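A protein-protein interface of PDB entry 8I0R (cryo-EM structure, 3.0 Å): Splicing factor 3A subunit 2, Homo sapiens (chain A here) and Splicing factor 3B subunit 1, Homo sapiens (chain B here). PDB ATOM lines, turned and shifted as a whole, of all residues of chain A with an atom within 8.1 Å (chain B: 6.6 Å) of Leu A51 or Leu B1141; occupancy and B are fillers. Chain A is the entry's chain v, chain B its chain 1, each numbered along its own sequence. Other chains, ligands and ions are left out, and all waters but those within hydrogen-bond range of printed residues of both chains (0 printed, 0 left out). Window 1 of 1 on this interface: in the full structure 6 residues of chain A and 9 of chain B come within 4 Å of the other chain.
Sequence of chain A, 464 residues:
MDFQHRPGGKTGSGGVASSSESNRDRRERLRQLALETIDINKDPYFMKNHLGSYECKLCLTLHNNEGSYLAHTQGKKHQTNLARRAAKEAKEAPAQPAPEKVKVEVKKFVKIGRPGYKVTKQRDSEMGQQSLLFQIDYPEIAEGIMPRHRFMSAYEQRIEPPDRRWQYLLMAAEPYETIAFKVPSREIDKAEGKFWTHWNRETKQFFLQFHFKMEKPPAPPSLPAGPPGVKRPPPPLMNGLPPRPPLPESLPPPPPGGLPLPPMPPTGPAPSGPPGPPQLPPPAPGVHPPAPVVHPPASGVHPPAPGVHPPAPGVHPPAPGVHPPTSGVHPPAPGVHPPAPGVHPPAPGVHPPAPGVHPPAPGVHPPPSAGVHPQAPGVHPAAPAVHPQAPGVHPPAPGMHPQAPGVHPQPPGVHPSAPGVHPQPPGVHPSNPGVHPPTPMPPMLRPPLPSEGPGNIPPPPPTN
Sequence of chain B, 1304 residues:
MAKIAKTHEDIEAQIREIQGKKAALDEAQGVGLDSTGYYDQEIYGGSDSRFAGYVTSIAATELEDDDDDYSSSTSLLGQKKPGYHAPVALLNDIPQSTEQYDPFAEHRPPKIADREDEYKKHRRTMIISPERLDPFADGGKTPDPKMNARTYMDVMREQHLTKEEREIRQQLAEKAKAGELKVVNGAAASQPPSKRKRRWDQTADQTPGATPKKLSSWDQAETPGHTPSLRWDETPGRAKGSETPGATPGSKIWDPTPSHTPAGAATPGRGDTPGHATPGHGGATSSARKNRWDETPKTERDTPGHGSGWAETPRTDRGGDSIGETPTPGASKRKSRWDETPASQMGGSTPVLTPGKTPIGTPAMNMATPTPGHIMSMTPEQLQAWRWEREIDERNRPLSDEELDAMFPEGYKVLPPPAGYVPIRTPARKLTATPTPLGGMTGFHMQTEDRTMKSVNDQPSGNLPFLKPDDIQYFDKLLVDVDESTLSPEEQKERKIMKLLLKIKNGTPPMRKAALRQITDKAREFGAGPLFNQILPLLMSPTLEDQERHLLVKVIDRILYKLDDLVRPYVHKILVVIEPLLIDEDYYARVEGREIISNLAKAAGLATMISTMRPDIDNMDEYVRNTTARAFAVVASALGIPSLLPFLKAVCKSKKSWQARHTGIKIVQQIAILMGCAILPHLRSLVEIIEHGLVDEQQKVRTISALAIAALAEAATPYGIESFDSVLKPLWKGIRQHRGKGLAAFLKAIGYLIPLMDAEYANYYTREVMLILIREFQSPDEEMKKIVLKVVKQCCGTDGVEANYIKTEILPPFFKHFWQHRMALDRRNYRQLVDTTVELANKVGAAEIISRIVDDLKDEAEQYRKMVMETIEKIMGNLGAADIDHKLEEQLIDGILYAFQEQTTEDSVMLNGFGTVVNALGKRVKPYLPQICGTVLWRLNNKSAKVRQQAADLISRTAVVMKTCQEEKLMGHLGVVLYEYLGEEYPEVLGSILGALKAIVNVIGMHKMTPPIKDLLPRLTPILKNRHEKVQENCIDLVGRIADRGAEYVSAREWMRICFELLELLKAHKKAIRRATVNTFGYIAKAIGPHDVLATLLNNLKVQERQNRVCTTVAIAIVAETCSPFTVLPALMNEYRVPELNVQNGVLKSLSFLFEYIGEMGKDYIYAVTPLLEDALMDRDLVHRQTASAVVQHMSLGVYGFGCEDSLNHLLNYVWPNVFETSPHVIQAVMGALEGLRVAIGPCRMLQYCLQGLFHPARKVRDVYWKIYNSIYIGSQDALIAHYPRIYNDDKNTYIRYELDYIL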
ATOM      1  N   ARG A  27      24.625 -11.052  -4.533  1.00  0.00           N
ATOM      2  CA  ARG A  27      23.962 -12.324  -4.285  1.00  0.00           C
ATOM      3  C   ARG A  27      23.695 -13.066  -5.583  1.00  0.00           C
ATOM      4  O   ARG A  27      23.880 -14.286  -5.659  1.00  0.00           O
ATOM      5  CB  ARG A  27      22.672 -12.100  -3.509  1.00  0.00           C
ATOM      6  CG  ARG A  27      22.879 -12.092  -2.003  1.00  0.00           C
ATOM      7  CD  ARG A  27      21.785 -11.357  -1.248  1.00  0.00           C
ATOM      8  NE  ARG A  27      20.921 -12.257  -0.488  1.00  0.00           N
ATOM      9  CZ  ARG A  27      19.593 -12.255  -0.553  1.00  0.00           C
ATOM     10  NH1 ARG A  27      18.966 -11.391  -1.336  1.00  0.00           N
ATOM     11  NH2 ARG A  27      18.893 -13.113   0.167  1.00  0.00           N
ATOM     12  N   LYS A  48      17.511 -26.846  -6.295  1.00  0.00           N
ATOM     13  CA  LYS A  48      17.008 -25.544  -5.904  1.00  0.00           C
ATOM     14  C   LYS A  48      15.507 -25.653  -5.703  1.00  0.00           C
ATOM     15  O   LYS A  48      14.791 -26.058  -6.622  1.00  0.00           O
ATOM     16  CB  LYS A  48      17.322 -24.517  -6.977  1.00  0.00           C
ATOM     17  CG  LYS A  48      17.132 -23.108  -6.533  1.00  0.00           C
ATOM     18  CD  LYS A  48      17.534 -22.165  -7.627  1.00  0.00           C
ATOM     19  CE  LYS A  48      18.173 -20.928  -7.066  1.00  0.00           C
ATOM     20  NZ  LYS A  48      18.621 -20.060  -8.167  1.00  0.00           N
ATOM     21  N   ASN A  49      15.027 -25.289  -4.522  1.00  0.00           N
ATOM     22  CA  ASN A  49      13.597 -25.380  -4.292  1.00  0.00           C
ATOM     23  C   ASN A  49      12.925 -24.058  -4.629  1.00  0.00           C
ATOM     24  O   ASN A  49      13.567 -23.067  -4.969  1.00  0.00           O
ATOM     25  CB  ASN A  49      13.303 -25.779  -2.857  1.00  0.00           C
ATOM     26  CG  ASN A  49      13.987 -24.906  -1.878  1.00  0.00           C
ATOM     27  OD1 ASN A  49      14.766 -24.053  -2.251  1.00  0.00           O
ATOM     28  ND2 ASN A  49      13.713 -25.112  -0.609  1.00  0.00           N
ATOM     29  N   HIS A  50      11.602 -24.053  -4.532  1.00  0.00           N
ATOM     30  CA  HIS A  50      10.831 -22.938  -5.059  1.00  0.00           C
ATOM     31  C   HIS A  50      10.934 -21.687  -4.206  1.00  0.00           C
ATOM     32  O   HIS A  50      10.244 -20.709  -4.489  1.00  0.00           O
ATOM     33  CB  HIS A  50       9.372 -23.338  -5.204  1.00  0.00           C
ATOM     34  CG  HIS A  50       8.704 -23.649  -3.910  1.00  0.00           C
ATOM     35  ND1 HIS A  50       9.361 -24.235  -2.855  1.00  0.00           N
ATOM     36  CD2 HIS A  50       7.439 -23.430  -3.491  1.00  0.00           C
ATOM     37  CE1 HIS A  50       8.527 -24.378  -1.843  1.00  0.00           C
ATOM     38  NE2 HIS A  50       7.353 -23.899  -2.205  1.00  0.00           N
ATOM     39  N   LEU A  51      11.756 -21.687  -3.172  1.00  0.00           N
ATOM     40  CA  LEU A  51      12.035 -20.458  -2.459  1.00  0.00           C
ATOM     41  C   LEU A  51      13.440 -19.966  -2.692  1.00  0.00           C
ATOM     42  O   LEU A  51      13.893 -19.074  -1.974  1.00  0.00           O
ATOM     43  CB  LEU A  51      11.820 -20.632  -0.969  1.00  0.00           C
ATOM     44  CG  LEU A  51      10.503 -21.266  -0.589  1.00  0.00           C
ATOM     45  CD1 LEU A  51      10.756 -22.600   0.058  1.00  0.00           C
ATOM     46  CD2 LEU A  51       9.789 -20.355   0.326  1.00  0.00           C
ATOM     47  N   GLY A  52      14.144 -20.518  -3.665  1.00  0.00           N
ATOM     48  CA  GLY A  52      15.460 -20.033  -3.980  1.00  0.00           C
ATOM     49  C   GLY A  52      16.523 -20.382  -2.976  1.00  0.00           C
ATOM     50  O   GLY A  52      17.573 -19.736  -2.961  1.00  0.00           O
ATOM     51  N   SER A  53      16.279 -21.355  -2.121  1.00  0.00           N
ATOM     52  CA  SER A  53      17.329 -21.905  -1.300  1.00  0.00           C
ATOM     53  C   SER A  53      17.687 -23.259  -1.877  1.00  0.00           C
ATOM     54  O   SER A  53      17.210 -23.635  -2.943  1.00  0.00           O
ATOM     55  CB  SER A  53      16.887 -22.017   0.152  1.00  0.00           C
ATOM     56  OG  SER A  53      15.918 -23.031   0.307  1.00  0.00           O
ATOM     57  N   TYR A  54      18.554 -23.988  -1.199  1.00  0.00           N
ATOM     58  CA  TYR A  54      19.075 -25.206  -1.788  1.00  0.00           C
ATOM     59  C   TYR A  54      18.781 -26.391  -0.900  1.00  0.00           C
ATOM     60  O   TYR A  54      18.546 -26.232   0.296  1.00  0.00           O
ATOM     61  CB  TYR A  54      20.564 -25.064  -2.035  1.00  0.00           C
ATOM     62  CG  TYR A  54      20.835 -23.787  -2.750  1.00  0.00           C
ATOM     63  CD1 TYR A  54      20.620 -23.685  -4.104  1.00  0.00           C
ATOM     64  CD2 TYR A  54      21.244 -22.667  -2.068  1.00  0.00           C
ATOM     65  CE1 TYR A  54      20.844 -22.520  -4.761  1.00  0.00           C
ATOM     66  CE2 TYR A  54      21.458 -21.504  -2.715  1.00  0.00           C
ATOM     67  CZ  TYR A  54      21.261 -21.436  -4.061  1.00  0.00           C
ATOM     68  OH  TYR A  54      21.480 -20.265  -4.719  1.00  0.00           O
ATOM     69  N   GLU A  55      18.775 -27.569  -1.491  1.00  0.00           N
ATOM     70  CA  GLU A  55      18.553 -28.804  -0.773  1.00  0.00           C
ATOM     71  C   GLU A  55      19.550 -29.836  -1.242  1.00  0.00           C
ATOM     72  O   GLU A  55      19.924 -29.856  -2.416  1.00  0.00           O
ATOM     73  CB  GLU A  55      17.154 -29.312  -1.009  1.00  0.00           C
ATOM     74  CG  GLU A  55      16.138 -28.478  -0.329  1.00  0.00           C
ATOM     75  CD  GLU A  55      14.796 -28.581  -0.972  1.00  0.00           C
ATOM     76  OE1 GLU A  55      13.875 -27.872  -0.536  1.00  0.00           O
ATOM     77  OE2 GLU A  55      14.658 -29.370  -1.921  1.00  0.00           O
ATOM     78  N   LEU A  62      18.479 -28.605   4.175  1.00  0.00           N
ATOM     79  CA  LEU A  62      18.166 -27.332   3.548  1.00  0.00           C
ATOM     80  C   LEU A  62      19.255 -26.325   3.835  1.00  0.00           C
ATOM     81  O   LEU A  62      19.814 -26.302   4.927  1.00  0.00           O
ATOM     82  CB  LEU A  62      16.856 -26.782   4.075  1.00  0.00           C
ATOM     83  CG  LEU A  62      15.676 -27.711   3.969  1.00  0.00           C
ATOM     84  CD1 LEU A  62      14.834 -27.508   5.169  1.00  0.00           C
ATOM     85  CD2 LEU A  62      14.908 -27.365   2.746  1.00  0.00           C
ATOM     86  N   HIS A  63      19.527 -25.463   2.865  1.00  0.00           N
ATOM     87  CA  HIS A  63      20.633 -24.530   2.958  1.00  0.00           C
ATOM     88  C   HIS A  63      20.205 -23.150   2.508  1.00  0.00           C
ATOM     89  O   HIS A  63      19.545 -23.007   1.477  1.00  0.00           O
ATOM     90  CB  HIS A  63      21.791 -25.012   2.120  1.00  0.00           C
ATOM     91  CG  HIS A  63      22.216 -26.402   2.440  1.00  0.00           C
ATOM     92  ND1 HIS A  63      22.685 -26.765   3.679  1.00  0.00           N
ATOM     93  CD2 HIS A  63      22.239 -27.519   1.688  1.00  0.00           C
ATOM     94  CE1 HIS A  63      22.984 -28.047   3.675  1.00  0.00           C
ATOM     95  NE2 HIS A  63      22.715 -28.529   2.480  1.00  0.00           N
ATOM     96  N   ASN A  64      20.617 -22.144   3.271  1.00  0.00           N
ATOM     97  CA  ASN A  64      20.324 -20.754   2.966  1.00  0.00           C
ATOM     98  C   ASN A  64      21.192 -20.246   1.836  1.00  0.00           C
ATOM     99  O   ASN A  64      20.683 -19.676   0.872  1.00  0.00           O
ATOM    100  CB  ASN A  64      20.555 -19.884   4.189  1.00  0.00           C
ATOM    101  CG  ASN A  64      19.802 -20.349   5.369  1.00  0.00           C
ATOM    102  OD1 ASN A  64      18.757 -20.971   5.240  1.00  0.00           O
ATOM    103  ND2 ASN A  64      20.322 -20.064   6.544  1.00  0.00           N
ATOM    104  N   VAL B1138       7.285 -16.009  -8.665  1.00  0.00           N
ATOM    105  CA  VAL B1138       8.724 -15.964  -8.878  1.00  0.00           C
ATOM    106  C   VAL B1138       9.377 -16.635  -7.679  1.00  0.00           C
ATOM    107  O   VAL B1138       8.901 -16.496  -6.548  1.00  0.00           O
ATOM    108  CB  VAL B1138       9.235 -14.532  -9.105  1.00  0.00           C
ATOM    109  CG1 VAL B1138       8.213 -13.708  -9.840  1.00  0.00           C
ATOM    110  CG2 VAL B1138       9.653 -13.883  -7.848  1.00  0.00           C
ATOM    111  N   PRO B1139      10.438 -17.373  -7.882  1.00  0.00           N
ATOM    112  CA  PRO B1139      10.904 -18.324  -6.870  1.00  0.00           C
ATOM    113  C   PRO B1139      11.599 -17.773  -5.638  1.00  0.00           C
ATOM    114  O   PRO B1139      12.384 -18.517  -5.056  1.00  0.00           O
ATOM    115  CB  PRO B1139      11.870 -19.213  -7.657  1.00  0.00           C
ATOM    116  CG  PRO B1139      12.056 -18.568  -8.946  1.00  0.00           C
ATOM    117  CD  PRO B1139      10.856 -17.788  -9.223  1.00  0.00           C
ATOM    118  N   GLU B1140      11.425 -16.523  -5.231  1.00  0.00           N
ATOM    119  CA  GLU B1140      12.109 -16.102  -4.019  1.00  0.00           C
ATOM    120  C   GLU B1140      11.210 -16.014  -2.796  1.00  0.00           C
ATOM    121  O   GLU B1140      10.049 -15.601  -2.864  1.00  0.00           O
ATOM    122  CB  GLU B1140      12.798 -14.767  -4.221  1.00  0.00           C
ATOM    123  CG  GLU B1140      14.002 -14.873  -5.085  1.00  0.00           C
ATOM    124  CD  GLU B1140      14.483 -13.534  -5.518  1.00  0.00           C
ATOM    125  OE1 GLU B1140      14.010 -12.546  -4.934  1.00  0.00           O
ATOM    126  OE2 GLU B1140      15.330 -13.467  -6.426  1.00  0.00           O
ATOM    127  N   LEU B1141      11.797 -16.361  -1.659  1.00  0.00           N
ATOM    128  CA  LEU B1141      11.224 -16.206  -0.335  1.00  0.00           C
ATOM    129  C   LEU B1141      10.745 -14.795  -0.087  1.00  0.00           C
ATOM    130  O   LEU B1141       9.605 -14.578   0.332  1.00  0.00           O
ATOM    131  CB  LEU B1141      12.270 -16.550   0.714  1.00  0.00           C
ATOM    132  CG  LEU B1141      11.901 -16.680   2.184  1.00  0.00           C
ATOM    133  CD1 LEU B1141      11.147 -17.932   2.448  1.00  0.00           C
ATOM    134  CD2 LEU B1141      13.150 -16.647   3.007  1.00  0.00           C
ATOM    135  N   ASN B1142      11.629 -13.828  -0.296  1.00  0.00           N
ATOM    136  CA  ASN B1142      11.309 -12.475   0.107  1.00  0.00           C
ATOM    137  C   ASN B1142      10.236 -11.862  -0.752  1.00  0.00           C
ATOM    138  O   ASN B1142       9.444 -11.075  -0.244  1.00  0.00           O
ATOM    139  CB  ASN B1142      12.551 -11.611   0.087  1.00  0.00           C
ATOM    140  CG  ASN B1142      13.465 -11.917   1.217  1.00  0.00           C
ATOM    141  OD1 ASN B1142      14.611 -11.502   1.229  1.00  0.00           O
ATOM    142  ND2 ASN B1142      12.968 -12.652   2.186  1.00  0.00           N
ATOM    143  N   VAL B1143      10.120 -12.245  -2.018  1.00  0.00           N
ATOM    144  CA  VAL B1143       9.037 -11.637  -2.765  1.00  0.00           C
ATOM    145  C   VAL B1143       7.733 -12.355  -2.497  1.00  0.00           C
ATOM    146  O   VAL B1143       6.675 -11.723  -2.501  1.00  0.00           O
ATOM    147  CB  VAL B1143       9.332 -11.560  -4.266  1.00  0.00           C
ATOM    148  CG1 VAL B1143      10.758 -11.845  -4.534  1.00  0.00           C
ATOM    149  CG2 VAL B1143       8.421 -12.458  -5.024  1.00  0.00           C
ATOM    150  N   GLN B1144       7.751 -13.657  -2.222  1.00  0.00           N
ATOM    151  CA  GLN B1144       6.490 -14.294  -1.867  1.00  0.00           C
ATOM    152  C   GLN B1144       5.939 -13.743  -0.558  1.00  0.00           C
ATOM    153  O   GLN B1144       4.745 -13.435  -0.453  1.00  0.00           O
ATOM    154  CB  GLN B1144       6.675 -15.795  -1.810  1.00  0.00           C
ATOM    155  CG  GLN B1144       6.968 -16.337  -3.165  1.00  0.00           C
ATOM    156  CD  GLN B1144       7.068 -17.820  -3.204  1.00  0.00           C
ATOM    157  OE1 GLN B1144       7.357 -18.465  -2.218  1.00  0.00           O
ATOM    158  NE2 GLN B1144       6.836 -18.376  -4.365  1.00  0.00           N
ATOM    159  N   ASN B1145       6.793 -13.554   0.443  1.00  0.00           N
ATOM    160  CA  ASN B1145       6.310 -12.899   1.653  1.00  0.00           C
ATOM    161  C   ASN B1145       5.991 -11.433   1.421  1.00  0.00           C
ATOM    162  O   ASN B1145       5.168 -10.866   2.138  1.00  0.00           O
ATOM    163  CB  ASN B1145       7.321 -13.013   2.773  1.00  0.00           C
ATOM    164  CG  ASN B1145       7.511 -14.405   3.218  1.00  0.00           C
ATOM    165  OD1 ASN B1145       6.839 -15.302   2.748  1.00  0.00           O
ATOM    166  ND2 ASN B1145       8.417 -14.605   4.150  1.00  0.00           N
ATOM    167  N   GLY B1146       6.607 -10.800   0.436  1.00  0.00           N
ATOM    168  CA  GLY B1146       6.222  -9.443   0.132  1.00  0.00           C
ATOM    169  C   GLY B1146       4.799  -9.348  -0.358  1.00  0.00           C
ATOM    170  O   GLY B1146       4.049  -8.475   0.065  1.00  0.00           O
ATOM    171  N   ASP B1179       2.666 -25.396   3.590  1.00  0.00           N
ATOM    172  CA  ASP B1179       3.867 -24.605   3.847  1.00  0.00           C
ATOM    173  C   ASP B1179       4.653 -24.302   2.601  1.00  0.00           C
ATOM    174  O   ASP B1179       4.758 -25.103   1.677  1.00  0.00           O
ATOM    175  CB  ASP B1179       4.789 -25.325   4.839  1.00  0.00           C
ATOM    176  CG  ASP B1179       6.279 -25.288   4.479  1.00  0.00           C
ATOM    177  OD1 ASP B1179       7.049 -24.568   5.136  1.00  0.00           O
ATOM    178  OD2 ASP B1179       6.699 -26.040   3.591  1.00  0.00           O
ATOM    179  N   ARG B1180       5.235 -23.133   2.607  1.00  0.00           N
ATOM    180  CA  ARG B1180       6.510 -22.925   1.946  1.00  0.00           C
ATOM    181  C   ARG B1180       7.591 -22.483   2.926  1.00  0.00           C
ATOM    182  O   ARG B1180       8.773 -22.502   2.583  1.00  0.00           O
ATOM    183  CB  ARG B1180       6.348 -21.905   0.816  1.00  0.00           C
ATOM    184  N   ASP B1181       7.209 -22.120   4.151  1.00  0.00           N
ATOM    185  CA  ASP B1181       8.074 -21.628   5.209  1.00  0.00           C
ATOM    186  C   ASP B1181       7.198 -21.355   6.422  1.00  0.00           C
ATOM    187  O   ASP B1181       5.988 -21.263   6.284  1.00  0.00           O
ATOM    188  CB  ASP B1181       8.806 -20.357   4.775  1.00  0.00           C
ATOM    189  CG  ASP B1181       9.969 -20.036   5.659  1.00  0.00           C
ATOM    190  OD1 ASP B1181      10.629 -20.987   6.110  1.00  0.00           O
ATOM    191  OD2 ASP B1181      10.227 -18.848   5.914  1.00  0.00           O
ATOM    192  N   VAL B1183       7.227 -18.491   7.829  1.00  0.00           N
ATOM    193  CA  VAL B1183       6.757 -17.129   7.644  1.00  0.00           C
ATOM    194  C   VAL B1183       5.644 -17.069   6.613  1.00  0.00           C
ATOM    195  O   VAL B1183       4.796 -16.178   6.662  1.00  0.00           O
ATOM    196  CB  VAL B1183       7.923 -16.210   7.273  1.00  0.00           C
ATOM    197  CG1 VAL B1183       7.461 -14.790   7.268  1.00  0.00           C
ATOM    198  CG2 VAL B1183       9.030 -16.377   8.256  1.00  0.00           C
ATOM    199  N   HIS B1184       5.599 -18.013   5.690  1.00  0.00           N
ATOM    200  CA  HIS B1184       4.479 -18.083   4.770  1.00  0.00           C
ATOM    201  C   HIS B1184       3.180 -18.283   5.512  1.00  0.00           C
ATOM    202  O   HIS B1184       2.187 -17.609   5.245  1.00  0.00           O
ATOM    203  CB  HIS B1184       4.673 -19.214   3.781  1.00  0.00           C
ATOM    204  CG  HIS B1184       5.483 -18.833   2.597  1.00  0.00           C
ATOM    205  ND1 HIS B1184       5.008 -18.925   1.314  1.00  0.00           N
ATOM    206  CD2 HIS B1184       6.726 -18.317   2.506  1.00  0.00           C
ATOM    207  CE1 HIS B1184       5.937 -18.508   0.478  1.00  0.00           C
ATOM    208  NE2 HIS B1184       6.989 -18.132   1.177  1.00  0.00           N
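The backbone carbonyl oxygen (O) of Pro B1139 sits close to the backbone carbonyl oxygen (O) of Leu A51, at 3.5 Å.
The backbone NH (N) of Gly A52 is in hydrogen-bond range of the backbone carbonyl oxygen (O) of Pro B1139.
O of His A50 lies close to O of Pro B1139, 3.1 Å away.
N of Leu B1141 is in hydrogen-bond range of O of Leu A51, 3.4 Å away.
OD1 of Asn B1145 sits close to NE2 of His B1184 (3.2 Å).
The side-chain amide oxygen (OE1) of Gln B1144 sits close to a ring nitrogen (NE2) of His B1184, at 3.4 Å.
His A50 touches Arg B1180 (NE2 to CB, 3.8 Å).
Gln B1144 touches Leu A51.
Arg B1180 touches Leu A51 (O to CD1, 3.2 Å).
His B1184 touches Leu A51 (NE2 to CD2, 3.7 Å).
Of the printed residues of chain B, Leu A51 touches Pro B1139 (3.0 Å), Leu B1141 (3.4 Å), Gln B1144 (3.99 Å), Arg B1180 (3.2 Å) and His B1184 (3.7 Å).
Leu B1141 touches just one residue of chain A: Leu A51.
Of the printed residues of chain B, Gly A52 touches Pro B1139.
Printed residues of chain A within 4 Å of Arg B1180: His A50 and Leu A51.
Printed residues of chain B within 4 Å of His A50: Pro B1139 (3.1 Å) and Arg B1180 (3.8 Å).
Asn B1145 touches none of the printed residues of chain A.
The nearest printed residue of chain B that does not touch Leu A51 is Glu B1140 (4.02 Å).
The nearest printed residue of chain A that does not touch His B1184 is His A50 (6.2 Å).
Of the 12 printed residues of chain A, 3 touch a printed residue of chain B.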
